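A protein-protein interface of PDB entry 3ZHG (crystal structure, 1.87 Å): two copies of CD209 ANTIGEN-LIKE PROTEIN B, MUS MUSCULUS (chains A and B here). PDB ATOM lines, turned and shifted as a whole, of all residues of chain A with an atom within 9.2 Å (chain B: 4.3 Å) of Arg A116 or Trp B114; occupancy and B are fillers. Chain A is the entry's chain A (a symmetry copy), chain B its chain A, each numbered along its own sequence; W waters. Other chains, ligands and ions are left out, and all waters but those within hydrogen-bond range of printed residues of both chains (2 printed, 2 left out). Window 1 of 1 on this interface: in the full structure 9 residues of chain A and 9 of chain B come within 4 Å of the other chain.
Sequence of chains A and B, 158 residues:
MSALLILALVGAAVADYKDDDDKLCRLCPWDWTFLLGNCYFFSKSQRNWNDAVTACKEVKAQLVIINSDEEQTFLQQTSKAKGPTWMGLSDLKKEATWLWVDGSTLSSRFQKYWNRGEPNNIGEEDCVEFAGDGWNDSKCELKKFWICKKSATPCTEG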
ATOM      1  N   SER A 108     -37.036  -4.860 -22.840  1.00  0.00           N
ATOM      2  CA  SER A 108     -37.130  -5.187 -21.432  1.00  0.00           C
ATOM      3  C   SER A 108     -36.253  -6.369 -21.122  1.00  0.00           C
ATOM      4  O   SER A 108     -35.648  -6.426 -20.060  1.00  0.00           O
ATOM      5  CB  SER A 108     -38.576  -5.485 -21.031  1.00  0.00           C
ATOM      6  OG  SER A 108     -39.304  -4.271 -20.921  1.00  0.00           O
ATOM      7  N   GLN A 111     -32.563  -5.652 -20.150  1.00  0.00           N
ATOM      8  CA  GLN A 111     -32.198  -4.773 -19.052  1.00  0.00           C
ATOM      9  C   GLN A 111     -31.508  -5.527 -17.937  1.00  0.00           C
ATOM     10  O   GLN A 111     -30.858  -4.922 -17.074  1.00  0.00           O
ATOM     11  CB  GLN A 111     -33.397  -3.967 -18.566  1.00  0.00           C
ATOM     12  CG  GLN A 111     -33.999  -3.159 -19.701  1.00  0.00           C
ATOM     13  CD  GLN A 111     -34.138  -1.704 -19.360  1.00  0.00           C
ATOM     14  OE1 GLN A 111     -33.152  -0.945 -19.345  1.00  0.00           O
ATOM     15  NE2 GLN A 111     -35.373  -1.291 -19.080  1.00  0.00           N
ATOM     16  N   LYS A 112     -31.611  -6.851 -17.979  1.00  0.00           N
ATOM     17  CA  LYS A 112     -30.905  -7.704 -17.025  1.00  0.00           C
ATOM     18  C   LYS A 112     -29.394  -7.687 -17.208  1.00  0.00           C
ATOM     19  O   LYS A 112     -28.658  -8.145 -16.327  1.00  0.00           O
ATOM     20  CB  LYS A 112     -31.400  -9.142 -17.112  1.00  0.00           C
ATOM     21  CG  LYS A 112     -31.092  -9.830 -18.416  1.00  0.00           C
ATOM     22  CD  LYS A 112     -31.781 -11.182 -18.474  1.00  0.00           C
ATOM     23  CE  LYS A 112     -31.454 -11.888 -19.777  1.00  0.00           C
ATOM     24  NZ  LYS A 112     -32.460 -12.924 -20.141  1.00  0.00           N
ATOM     25  N   TYR A 113     -28.927  -7.162 -18.342  1.00  0.00           N
ATOM     26  CA  TYR A 113     -27.491  -7.153 -18.622  1.00  0.00           C
ATOM     27  C   TYR A 113     -26.775  -6.040 -17.883  1.00  0.00           C
ATOM     28  O   TYR A 113     -25.568  -6.123 -17.664  1.00  0.00           O
ATOM     29  CB  TYR A 113     -27.209  -7.089 -20.130  1.00  0.00           C
ATOM     30  CG  TYR A 113     -27.725  -8.307 -20.863  1.00  0.00           C
ATOM     31  CD1 TYR A 113     -27.422  -9.584 -20.416  1.00  0.00           C
ATOM     32  CD2 TYR A 113     -28.523  -8.181 -21.998  1.00  0.00           C
ATOM     33  CE1 TYR A 113     -27.905 -10.715 -21.073  1.00  0.00           C
ATOM     34  CE2 TYR A 113     -28.984  -9.305 -22.677  1.00  0.00           C
ATOM     35  CZ  TYR A 113     -28.680 -10.562 -22.200  1.00  0.00           C
ATOM     36  OH  TYR A 113     -29.160 -11.676 -22.851  1.00  0.00           O
ATOM     37  N   TRP A 114     -27.511  -5.006 -17.485  1.00  0.00           N
ATOM     38  CA  TRP A 114     -26.937  -3.955 -16.645  1.00  0.00           C
ATOM     39  C   TRP A 114     -26.314  -4.541 -15.390  1.00  0.00           C
ATOM     40  O   TRP A 114     -26.911  -5.406 -14.745  1.00  0.00           O
ATOM     41  CB  TRP A 114     -28.009  -2.970 -16.188  1.00  0.00           C
ATOM     42  CG  TRP A 114     -28.561  -2.045 -17.236  1.00  0.00           C
ATOM     43  CD1 TRP A 114     -29.835  -2.038 -17.724  1.00  0.00           C
ATOM     44  CD2 TRP A 114     -27.874  -0.972 -17.896  1.00  0.00           C
ATOM     45  NE1 TRP A 114     -29.983  -1.031 -18.650  1.00  0.00           N
ATOM     46  CE2 TRP A 114     -28.791  -0.367 -18.779  1.00  0.00           C
ATOM     47  CE3 TRP A 114     -26.576  -0.465 -17.829  1.00  0.00           C
ATOM     48  CZ2 TRP A 114     -28.452   0.717 -19.586  1.00  0.00           C
ATOM     49  CZ3 TRP A 114     -26.243   0.615 -18.626  1.00  0.00           C
ATOM     50  CH2 TRP A 114     -27.179   1.194 -19.494  1.00  0.00           C
ATOM     51  N   ASN A 115     -25.132  -4.048 -15.015  1.00  0.00           N
ATOM     52  CA  ASN A 115     -24.538  -4.417 -13.736  1.00  0.00           C
ATOM     53  C   ASN A 115     -25.405  -3.904 -12.597  1.00  0.00           C
ATOM     54  O   ASN A 115     -26.203  -2.976 -12.782  1.00  0.00           O
ATOM     55  CB  ASN A 115     -23.150  -3.803 -13.599  1.00  0.00           C
ATOM     56  CG  ASN A 115     -22.065  -4.669 -14.204  1.00  0.00           C
ATOM     57  OD1 ASN A 115     -22.123  -5.894 -14.114  1.00  0.00           O
ATOM     58  ND2 ASN A 115     -21.055  -4.036 -14.808  1.00  0.00           N
ATOM     59  N   ARG A 116     -25.263  -4.504 -11.417  1.00  0.00           N
ATOM     60  CA  ARG A 116     -25.950  -3.998 -10.244  1.00  0.00           C
ATOM     61  C   ARG A 116     -25.522  -2.553 -10.019  1.00  0.00           C
ATOM     62  O   ARG A 116     -24.336  -2.244 -10.053  1.00  0.00           O
ATOM     63  CB  ARG A 116     -25.609  -4.849  -9.023  1.00  0.00           C
ATOM     64  CG  ARG A 116     -26.576  -4.678  -7.871  1.00  0.00           C
ATOM     65  CD  ARG A 116     -26.006  -5.286  -6.615  1.00  0.00           C
ATOM     66  NE  ARG A 116     -24.971  -4.453  -6.012  1.00  0.00           N
ATOM     67  CZ  ARG A 116     -23.688  -4.792  -5.927  1.00  0.00           C
ATOM     68  NH1 ARG A 116     -23.267  -5.954  -6.414  1.00  0.00           N
ATOM     69  NH2 ARG A 116     -22.828  -3.969  -5.346  1.00  0.00           N
ATOM     70  N   GLY A 117     -26.486  -1.662  -9.812  1.00  0.00           N
ATOM     71  CA  GLY A 117     -26.157  -0.259  -9.608  1.00  0.00           C
ATOM     72  C   GLY A 117     -26.095   0.557 -10.891  1.00  0.00           C
ATOM     73  O   GLY A 117     -25.811   1.754 -10.856  1.00  0.00           O
ATOM     74  N   GLU A 118     -26.352  -0.084 -12.028  1.00  0.00           N
ATOM     75  CA  GLU A 118     -26.357   0.605 -13.316  1.00  0.00           C
ATOM     76  C   GLU A 118     -27.720   0.457 -13.969  1.00  0.00           C
ATOM     77  O   GLU A 118     -28.404  -0.538 -13.762  1.00  0.00           O
ATOM     78  CB  GLU A 118     -25.287   0.018 -14.241  1.00  0.00           C
ATOM     79  CG  GLU A 118     -23.878   0.028 -13.653  1.00  0.00           C
ATOM     80  CD  GLU A 118     -23.208   1.390 -13.735  1.00  0.00           C
ATOM     81  OE1 GLU A 118     -23.501   2.166 -14.679  1.00  0.00           O
ATOM     82  OE2 GLU A 118     -22.369   1.689 -12.855  1.00  0.00           O
ATOM     83  N   PRO A 119     -28.119   1.444 -14.774  1.00  0.00           N
ATOM     84  CA  PRO A 119     -27.363   2.661 -15.067  1.00  0.00           C
ATOM     85  C   PRO A 119     -27.483   3.693 -13.961  1.00  0.00           C
ATOM     86  O   PRO A 119     -28.539   3.776 -13.331  1.00  0.00           O
ATOM     87  CB  PRO A 119     -28.048   3.185 -16.329  1.00  0.00           C
ATOM     88  CG  PRO A 119     -29.433   2.683 -16.230  1.00  0.00           C
ATOM     89  CD  PRO A 119     -29.312   1.315 -15.627  1.00  0.00           C
ATOM     90  N   ASN A 120     -26.437   4.482 -13.732  1.00  0.00           N
ATOM     91  CA  ASN A 120     -26.526   5.554 -12.736  1.00  0.00           C
ATOM     92  C   ASN A 120     -25.958   6.855 -13.281  1.00  0.00           C
ATOM     93  O   ASN A 120     -25.746   6.990 -14.484  1.00  0.00           O
ATOM     94  CB  ASN A 120     -25.803   5.161 -11.445  1.00  0.00           C
ATOM     95  CG  ASN A 120     -24.330   4.970 -11.653  1.00  0.00           C
ATOM     96  OD1 ASN A 120     -23.848   5.038 -12.783  1.00  0.00           O
ATOM     97  ND2 ASN A 120     -23.597   4.714 -10.571  1.00  0.00           N
ATOM     98  N   ALA A 131     -18.445  -3.760 -19.035  1.00  0.00           N
ATOM     99  CA  ALA A 131     -17.486  -3.647 -17.939  1.00  0.00           C
ATOM    100  C   ALA A 131     -17.598  -4.894 -17.085  1.00  0.00           C
ATOM    101  O   ALA A 131     -18.631  -5.119 -16.454  1.00  0.00           O
ATOM    102  CB  ALA A 131     -17.791  -2.429 -17.097  1.00  0.00           C
ATOM    103  N   ASP A 133     -18.644  -8.231 -16.113  1.00  0.00           N
ATOM    104  CA  ASP A 133     -19.638  -9.211 -16.521  1.00  0.00           C
ATOM    105  C   ASP A 133     -20.977  -8.594 -16.904  1.00  0.00           C
ATOM    106  O   ASP A 133     -21.941  -9.315 -17.109  1.00  0.00           O
ATOM    107  CB  ASP A 133     -19.890 -10.236 -15.408  1.00  0.00           C
ATOM    108  CG  ASP A 133     -18.668 -11.079 -15.088  1.00  0.00           C
ATOM    109  OD1 ASP A 133     -18.090 -11.680 -16.021  1.00  0.00           O
ATOM    110  OD2 ASP A 133     -18.299 -11.149 -13.893  1.00  0.00           O
ATOM    111  N   GLY A 134     -21.049  -7.274 -16.992  1.00  0.00           N
ATOM    112  CA  GLY A 134     -22.288  -6.633 -17.385  1.00  0.00           C
ATOM    113  C   GLY A 134     -22.049  -5.264 -17.984  1.00  0.00           C
ATOM    114  O   GLY A 134     -20.930  -4.962 -18.370  1.00  0.00           O
ATOM    115  N   TRP A 135     -23.098  -4.446 -18.059  1.00  0.00           N
ATOM    116  CA  TRP A 135     -23.026  -3.131 -18.679  1.00  0.00           C
ATOM    117  C   TRP A 135     -23.013  -2.022 -17.645  1.00  0.00           C
ATOM    118  O   TRP A 135     -23.762  -2.075 -16.661  1.00  0.00           O
ATOM    119  CB  TRP A 135     -24.232  -2.890 -19.590  1.00  0.00           C
ATOM    120  CG  TRP A 135     -24.512  -3.952 -20.618  1.00  0.00           C
ATOM    121  CD1 TRP A 135     -23.750  -5.041 -20.907  1.00  0.00           C
ATOM    122  CD2 TRP A 135     -25.653  -4.017 -21.495  1.00  0.00           C
ATOM    123  NE1 TRP A 135     -24.338  -5.779 -21.918  1.00  0.00           N
ATOM    124  CE2 TRP A 135     -25.511  -5.164 -22.289  1.00  0.00           C
ATOM    125  CE3 TRP A 135     -26.779  -3.200 -21.686  1.00  0.00           C
ATOM    126  CZ2 TRP A 135     -26.446  -5.527 -23.262  1.00  0.00           C
ATOM    127  CZ3 TRP A 135     -27.711  -3.565 -22.650  1.00  0.00           C
ATOM    128  CH2 TRP A 135     -27.535  -4.715 -23.427  1.00  0.00           C
ATOM    129  N   ASN A 136     -22.173  -1.016 -17.876  1.00  0.00           N
ATOM    130  CA  ASN A 136     -22.196   0.222 -17.109  1.00  0.00           C
ATOM    131  C   ASN A 136     -22.563   1.326 -18.067  1.00  0.00           C
ATOM    132  O   ASN A 136     -22.322   1.188 -19.265  1.00  0.00           O
ATOM    133  CB  ASN A 136     -20.801   0.556 -16.580  1.00  0.00           C
ATOM    134  CG  ASN A 136     -20.377  -0.324 -15.436  1.00  0.00           C
ATOM    135  OD1 ASN A 136     -21.080  -1.254 -15.062  1.00  0.00           O
ATOM    136  ND2 ASN A 136     -19.217  -0.027 -14.865  1.00  0.00           N
ATOM    137  N   ASP A 137     -23.122   2.431 -17.576  1.00  0.00           N
ATOM    138  CA  ASP A 137     -23.073   3.647 -18.380  1.00  0.00           C
ATOM    139  C   ASP A 137     -21.805   4.399 -17.979  1.00  0.00           C
ATOM    140  O   ASP A 137     -21.352   4.296 -16.827  1.00  0.00           O
ATOM    141  CB  ASP A 137     -24.343   4.496 -18.254  1.00  0.00           C
ATOM    142  CG  ASP A 137     -24.597   4.982 -16.840  1.00  0.00           C
ATOM    143  OD1 ASP A 137     -23.858   4.578 -15.922  1.00  0.00           O
ATOM    144  OD2 ASP A 137     -25.540   5.783 -16.658  1.00  0.00           O
ATOM    145  N   TRP B  98     -43.274  -4.316 -14.203  1.00  0.00           N
ATOM    146  CA  TRP B  98     -43.206  -4.429 -12.735  1.00  0.00           C
ATOM    147  C   TRP B  98     -43.964  -3.319 -12.027  1.00  0.00           C
ATOM    148  O   TRP B  98     -43.666  -2.139 -12.206  1.00  0.00           O
ATOM    149  CB  TRP B  98     -41.738  -4.468 -12.289  1.00  0.00           C
ATOM    150  CG  TRP B  98     -41.024  -5.609 -12.938  1.00  0.00           C
ATOM    151  CD1 TRP B  98     -40.327  -5.583 -14.121  1.00  0.00           C
ATOM    152  CD2 TRP B  98     -40.993  -6.966 -12.489  1.00  0.00           C
ATOM    153  NE1 TRP B  98     -39.850  -6.844 -14.413  1.00  0.00           N
ATOM    154  CE2 TRP B  98     -40.244  -7.701 -13.418  1.00  0.00           C
ATOM    155  CE3 TRP B  98     -41.507  -7.620 -11.358  1.00  0.00           C
ATOM    156  CZ2 TRP B  98     -40.008  -9.062 -13.268  1.00  0.00           C
ATOM    157  CZ3 TRP B  98     -41.273  -8.971 -11.222  1.00  0.00           C
ATOM    158  CH2 TRP B  98     -40.539  -9.679 -12.167  1.00  0.00           C
ATOM    159  N   LEU B 106     -42.810   0.947 -11.749  1.00  0.00           N
ATOM    160  CA  LEU B 106     -41.425   0.979 -11.307  1.00  0.00           C
ATOM    161  C   LEU B 106     -40.684   2.009 -12.145  1.00  0.00           C
ATOM    162  O   LEU B 106     -40.667   1.921 -13.359  1.00  0.00           O
ATOM    163  CB  LEU B 106     -40.793  -0.407 -11.491  1.00  0.00           C
ATOM    164  CG  LEU B 106     -39.313  -0.562 -11.127  1.00  0.00           C
ATOM    165  CD1 LEU B 106     -39.089  -0.335  -9.629  1.00  0.00           C
ATOM    166  CD2 LEU B 106     -38.820  -1.934 -11.536  1.00  0.00           C
ATOM    167  N   GLN B 111     -34.367   1.023 -11.607  1.00  0.00           N
ATOM    168  CA  GLN B 111     -34.040  -0.229 -12.267  1.00  0.00           C
ATOM    169  C   GLN B 111     -32.600  -0.628 -12.032  1.00  0.00           C
ATOM    170  O   GLN B 111     -32.223  -1.788 -12.244  1.00  0.00           O
ATOM    171  CB  GLN B 111     -34.408  -0.188 -13.745  1.00  0.00           C
ATOM    172  CG  GLN B 111     -35.882   0.126 -13.925  1.00  0.00           C
ATOM    173  CD  GLN B 111     -36.582  -0.876 -14.797  1.00  0.00           C
ATOM    174  OE1 GLN B 111     -36.876  -2.008 -14.375  1.00  0.00           O
ATOM    175  NE2 GLN B 111     -36.859  -0.471 -16.036  1.00  0.00           N
ATOM    176  N   LYS B 112     -31.805   0.322 -11.551  1.00  0.00           N
ATOM    177  CA  LYS B 112     -30.419   0.044 -11.180  1.00  0.00           C
ATOM    178  C   LYS B 112     -30.294  -0.858  -9.960  1.00  0.00           C
ATOM    179  O   LYS B 112     -29.209  -1.384  -9.687  1.00  0.00           O
ATOM    180  CB  LYS B 112     -29.656   1.337 -10.922  1.00  0.00           C
ATOM    181  CG  LYS B 112     -30.136   2.118  -9.728  1.00  0.00           C
ATOM    182  CD  LYS B 112     -29.440   3.467  -9.666  1.00  0.00           C
ATOM    183  CE  LYS B 112     -29.906   4.247  -8.451  1.00  0.00           C
ATOM    184  NZ  LYS B 112     -29.698   5.715  -8.593  1.00  0.00           N
ATOM    185  N   TYR B 113     -31.392  -1.041  -9.226  1.00  0.00           N
ATOM    186  CA  TYR B 113     -31.348  -1.850  -8.009  1.00  0.00           C
ATOM    187  C   TYR B 113     -31.376  -3.335  -8.312  1.00  0.00           C
ATOM    188  O   TYR B 113     -30.941  -4.140  -7.491  1.00  0.00           O
ATOM    189  CB  TYR B 113     -32.466  -1.462  -7.030  1.00  0.00           C
ATOM    190  CG  TYR B 113     -32.330  -0.039  -6.538  1.00  0.00           C
ATOM    191  CD1 TYR B 113     -31.126   0.423  -6.029  1.00  0.00           C
ATOM    192  CD2 TYR B 113     -33.404   0.847  -6.589  1.00  0.00           C
ATOM    193  CE1 TYR B 113     -30.982   1.737  -5.588  1.00  0.00           C
ATOM    194  CE2 TYR B 113     -33.278   2.153  -6.122  1.00  0.00           C
ATOM    195  CZ  TYR B 113     -32.063   2.588  -5.637  1.00  0.00           C
ATOM    196  OH  TYR B 113     -31.926   3.887  -5.204  1.00  0.00           O
ATOM    197  N   TRP B 114     -31.872  -3.704  -9.491  1.00  0.00           N
ATOM    198  CA  TRP B 114     -31.811  -5.098  -9.928  1.00  0.00           C
ATOM    199  C   TRP B 114     -30.385  -5.620  -9.885  1.00  0.00           C
ATOM    200  O   TRP B 114     -29.458  -4.933 -10.321  1.00  0.00           O
ATOM    201  CB  TRP B 114     -32.292  -5.244 -11.369  1.00  0.00           C
ATOM    202  CG  TRP B 114     -33.766  -5.072 -11.605  1.00  0.00           C
ATOM    203  CD1 TRP B 114     -34.366  -4.066 -12.304  1.00  0.00           C
ATOM    204  CD2 TRP B 114     -34.821  -5.947 -11.178  1.00  0.00           C
ATOM    205  NE1 TRP B 114     -35.728  -4.256 -12.335  1.00  0.00           N
ATOM    206  CE2 TRP B 114     -36.033  -5.399 -11.644  1.00  0.00           C
ATOM    207  CE3 TRP B 114     -34.860  -7.134 -10.447  1.00  0.00           C
ATOM    208  CZ2 TRP B 114     -37.268  -6.000 -11.404  1.00  0.00           C
ATOM    209  CZ3 TRP B 114     -36.085  -7.732 -10.215  1.00  0.00           C
ATOM    210  CH2 TRP B 114     -37.274  -7.162 -10.694  1.00  0.00           C
ATOM    211  N   ASN B 115     -30.205  -6.849  -9.397  1.00  0.00           N
ATOM    212  CA  ASN B 115     -28.906  -7.504  -9.476  1.00  0.00           C
ATOM    213  C   ASN B 115     -28.538  -7.746 -10.932  1.00  0.00           C
ATOM    214  O   ASN B 115     -29.413  -7.770 -11.807  1.00  0.00           O
ATOM    215  CB  ASN B 115     -28.945  -8.848  -8.758  1.00  0.00           C
ATOM    216  CG  ASN B 115     -28.648  -8.728  -7.278  1.00  0.00           C
ATOM    217  OD1 ASN B 115     -27.809  -7.925  -6.873  1.00  0.00           O
ATOM    218  ND2 ASN B 115     -29.321  -9.543  -6.461  1.00  0.00           N
ATOM    219  N   ARG B 116     -27.246  -7.922 -11.203  1.00  0.00           N
ATOM    220  CA  ARG B 116     -26.816  -8.289 -12.539  1.00  0.00           C
ATOM    221  C   ARG B 116     -27.494  -9.600 -12.921  1.00  0.00           C
ATOM    222  O   ARG B 116     -27.502 -10.546 -12.142  1.00  0.00           O
ATOM    223  CB  ARG B 116     -25.298  -8.444 -12.582  1.00  0.00           C
ATOM    224  CG  ARG B 116     -24.720  -8.404 -13.980  1.00  0.00           C
ATOM    225  CD  ARG B 116     -23.290  -8.878 -13.969  1.00  0.00           C
ATOM    226  NE  ARG B 116     -23.183 -10.328 -13.849  1.00  0.00           N
ATOM    227  CZ  ARG B 116     -22.671 -10.960 -12.797  1.00  0.00           C
ATOM    228  NH1 ARG B 116     -22.217 -10.271 -11.755  1.00  0.00           N
ATOM    229  NH2 ARG B 116     -22.606 -12.283 -12.792  1.00  0.00           N
ATOM    230  N   GLU B 118     -30.723  -9.873 -13.485  1.00  0.00           N
ATOM    231  CA  GLU B 118     -32.128  -9.801 -13.089  1.00  0.00           C
ATOM    232  C   GLU B 118     -32.767  -8.569 -13.706  1.00  0.00           C
ATOM    233  O   GLU B 118     -32.101  -7.565 -13.924  1.00  0.00           O
ATOM    234  CB  GLU B 118     -32.251  -9.725 -11.565  1.00  0.00           C
ATOM    235  CG  GLU B 118     -31.562 -10.870 -10.824  1.00  0.00           C
ATOM    236  CD  GLU B 118     -32.372 -12.156 -10.831  1.00  0.00           C
ATOM    237  OE1 GLU B 118     -33.627 -12.095 -10.867  1.00  0.00           O
ATOM    238  OE2 GLU B 118     -31.754 -13.243 -10.787  1.00  0.00           O
ATOM    239  N   PRO B 119     -34.072  -8.635 -13.980  1.00  0.00           N
ATOM    240  CA  PRO B 119     -34.931  -9.796 -13.753  1.00  0.00           C
ATOM    241  C   PRO B 119     -34.785 -10.842 -14.842  1.00  0.00           C
ATOM    242  O   PRO B 119     -34.557 -10.478 -15.997  1.00  0.00           O
ATOM    243  CB  PRO B 119     -36.334  -9.191 -13.814  1.00  0.00           C
ATOM    244  CG  PRO B 119     -36.189  -8.018 -14.699  1.00  0.00           C
ATOM    245  CD  PRO B 119     -34.843  -7.444 -14.372  1.00  0.00           C
ATOM    246  N   VAL B 128     -40.687  -9.932  -6.459  1.00  0.00           N
ATOM    247  CA  VAL B 128     -39.351  -9.398  -6.241  1.00  0.00           C
ATOM    248  C   VAL B 128     -38.898  -9.471  -4.780  1.00  0.00           C
ATOM    249  O   VAL B 128     -39.677  -9.209  -3.861  1.00  0.00           O
ATOM    250  CB  VAL B 128     -39.250  -7.952  -6.775  1.00  0.00           C
ATOM    251  CG1 VAL B 128     -37.836  -7.440  -6.663  1.00  0.00           C
ATOM    252  CG2 VAL B 128     -39.680  -7.917  -8.240  1.00  0.00           C
ATOM    253  N   ASP B 133     -27.183  -7.808  -2.274  1.00  0.00           N
ATOM    254  CA  ASP B 133     -27.043  -6.367  -2.407  1.00  0.00           C
ATOM    255  C   ASP B 133     -27.966  -5.761  -3.456  1.00  0.00           C
ATOM    256  O   ASP B 133     -27.833  -4.591  -3.778  1.00  0.00           O
ATOM    257  CB  ASP B 133     -25.601  -5.985  -2.766  1.00  0.00           C
ATOM    258  CG  ASP B 133     -24.603  -6.343  -1.679  1.00  0.00           C
ATOM    259  OD1 ASP B 133     -24.813  -5.941  -0.513  1.00  0.00           O
ATOM    260  OD2 ASP B 133     -23.598  -7.016  -2.003  1.00  0.00           O
ATOM    261  N   GLY B 134     -28.887  -6.544  -3.997  1.00  0.00           N
ATOM    262  CA  GLY B 134     -29.814  -6.013  -4.978  1.00  0.00           C
ATOM    263  C   GLY B 134     -31.092  -6.820  -5.037  1.00  0.00           C
ATOM    264  O   GLY B 134     -31.372  -7.577  -4.119  1.00  0.00           O
ATOM    265  N   TRP B 135     -31.861  -6.656  -6.114  1.00  0.00           N
ATOM    266  CA  TRP B 135     -33.152  -7.312  -6.265  1.00  0.00           C
ATOM    267  C   TRP B 135     -33.084  -8.465  -7.248  1.00  0.00           C
ATOM    268  O   TRP B 135     -32.449  -8.349  -8.305  1.00  0.00           O
ATOM    269  CB  TRP B 135     -34.205  -6.332  -6.786  1.00  0.00           C
ATOM    270  CG  TRP B 135     -34.347  -5.041  -6.025  1.00  0.00           C
ATOM    271  CD1 TRP B 135     -33.730  -4.697  -4.862  1.00  0.00           C
ATOM    272  CD2 TRP B 135     -35.167  -3.915  -6.390  1.00  0.00           C
ATOM    273  NE1 TRP B 135     -34.121  -3.430  -4.472  1.00  0.00           N
ATOM    274  CE2 TRP B 135     -35.004  -2.934  -5.403  1.00  0.00           C
ATOM    275  CE3 TRP B 135     -36.035  -3.654  -7.464  1.00  0.00           C
ATOM    276  CZ2 TRP B 135     -35.668  -1.705  -5.444  1.00  0.00           C
ATOM    277  CZ3 TRP B 135     -36.693  -2.430  -7.506  1.00  0.00           C
ATOM    278  CH2 TRP B 135     -36.507  -1.475  -6.501  1.00  0.00           C
ATOM    279  N   ASN B 136     -33.747  -9.566  -6.905  1.00  0.00           N
ATOM    280  CA  ASN B 136     -33.967 -10.672  -7.827  1.00  0.00           C
ATOM    281  C   ASN B 136     -35.456 -10.773  -8.044  1.00  0.00           C
ATOM    282  O   ASN B 136     -36.220 -10.352  -7.178  1.00  0.00           O
ATOM    283  CB  ASN B 136     -33.533 -11.996  -7.197  1.00  0.00           C
ATOM    284  CG  ASN B 136     -32.039 -12.153  -7.125  1.00  0.00           C
ATOM    285  OD1 ASN B 136     -31.292 -11.246  -7.472  1.00  0.00           O
ATOM    286  ND2 ASN B 136     -31.592 -13.319  -6.678  1.00  0.00           N
ATOM    287  N   ASP B 137     -35.895 -11.338  -9.167  1.00  0.00           N
ATOM    288  CA  ASP B 137     -37.264 -11.840  -9.200  1.00  0.00           C
ATOM    289  C   ASP B 137     -37.215 -13.304  -8.766  1.00  0.00           C
ATOM    290  O   ASP B 137     -36.206 -13.993  -8.991  1.00  0.00           O
ATOM    291  CB  ASP B 137     -37.941 -11.637 -10.560  1.00  0.00           C
ATOM    292  CG  ASP B 137     -37.240 -12.364 -11.690  1.00  0.00           C
ATOM    293  OD1 ASP B 137     -36.162 -12.943 -11.456  1.00  0.00           O
ATOM    294  OD2 ASP B 137     -37.785 -12.361 -12.815  1.00  0.00           O
HETATM  295  O   HOH W   1     -32.703  -4.604 -15.313  1.00  0.00           O
HETATM  296  O   HOH W   2     -31.442  -1.530 -14.680  1.00  0.00           O
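O of Lys B112 lies within hydrogen-bond range of N of Gly A117 (2.7 Å).
The side-chain amide nitrogen of Gln A111 lies close to the side-chain amide nitrogen of Gln B111 (3.5 Å).
The indole nitrogen (NE1) of Trp A114 lies within hydrogen-bond range of the side-chain amide oxygen (OE1) of Gln A111 (3.2 Å).
The side-chain amide oxygen (OD1) of Asn B115 sits close to the backbone NH (N) of Gly B134 (3.4 Å).
The side-chain amide oxygen (OD1) of Asn B136 lies within hydrogen-bond range of the side-chain amide nitrogen (ND2) of Asn B115 (2.8 Å).
The side-chain amide nitrogen of Asn A115 is in hydrogen-bond range of the side-chain amide oxygen of Asn A136 (2.8 Å).
The side-chain amide nitrogen of Asn A115 lies within hydrogen-bond range of the backbone carbonyl oxygen of Ala A131, 3.1 Å away.
The backbone NH (N) of Asn A115 is in hydrogen-bond range of the backbone carbonyl oxygen (O) of Trp A135.
Among the printed residues, merely in contact across the chains: Lys A112 with Arg B116 (3.9 Å), Lys A112 with Glu B118 (3.3 Å), Lys A112 with Pro B119 (3.6 Å), Trp A114 with Arg B116 (3.6 Å), Asn A115 with Arg B116 (3.2 Å), Arg A116 with Lys B112 (3.9 Å), Arg A116 with Trp B114 (3.6 Å), Arg A116 with Asn B115 (3.2 Å), Arg A116 with Arg B116 (3.96 Å), Arg A116 with Asp B133 (3.4 Å), Glu A118 with Lys B112 (3.3 Å), Pro A119 with Lys B112 (3.6 Å) and Asp A133 with Arg B116 (3.4 Å).
Printed residues of chain B within 4 Å of Gln A111: Gln B111 (3.5 Å).
Of the printed residues of chain B, Trp A114 touches Arg B116.
Printed residues of chain B within 4 Å of Arg A116: Lys B112, Trp B114, Asn B115, Arg B116 and Asp B133.
Of the printed residues of chain A, Trp B114 touches Arg A116.
Of the printed residues of chain A, Pro B119 touches Lys A112 (3.6 Å).
Asp B137 touches none of the printed residues of chain A.
The nearest printed residue of chain A that does not touch Trp B114 is Gly A117 (4.4 Å).
The nearest printed residue of chain B that does not touch Gly A117 is Trp B114 (4.4 Å).
Of the 17 printed residues of chain A, 9 touch a printed residue of chain B.
Of the 16 printed residues of chain B, 8 touch a printed residue of chain A.
Among the printed residues, 15 pairs touch across the chains.
Gln A111 touches its own counterpart, Gln B111.
Lys A112 touches Glu B118, and with the chains exchanged Glu A118 touches Lys B112.
Asn A115 touches Arg B116, and with the chains exchanged Arg A116 touches Asn B115.
Arg B116 touches its own counterpart, Arg A116.
Positions printed for both chains: 111, 112, 113, 114, 115, 116, 118, 119, 133, 134, 135, 136 and 137.
Of the 15 pairs that touch across the chains among the printed residues, 14 have their exchanged pair printed and touching as well.
Water W2 lies within hydrogen-bond range of O of Gln B111 (2.6 Å) and O of Glu A118 (3.3 Å).
Water W1 lies within hydrogen-bond range of O of Gln A111 (2.6 Å) and O of Glu B118 (3.3 Å).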
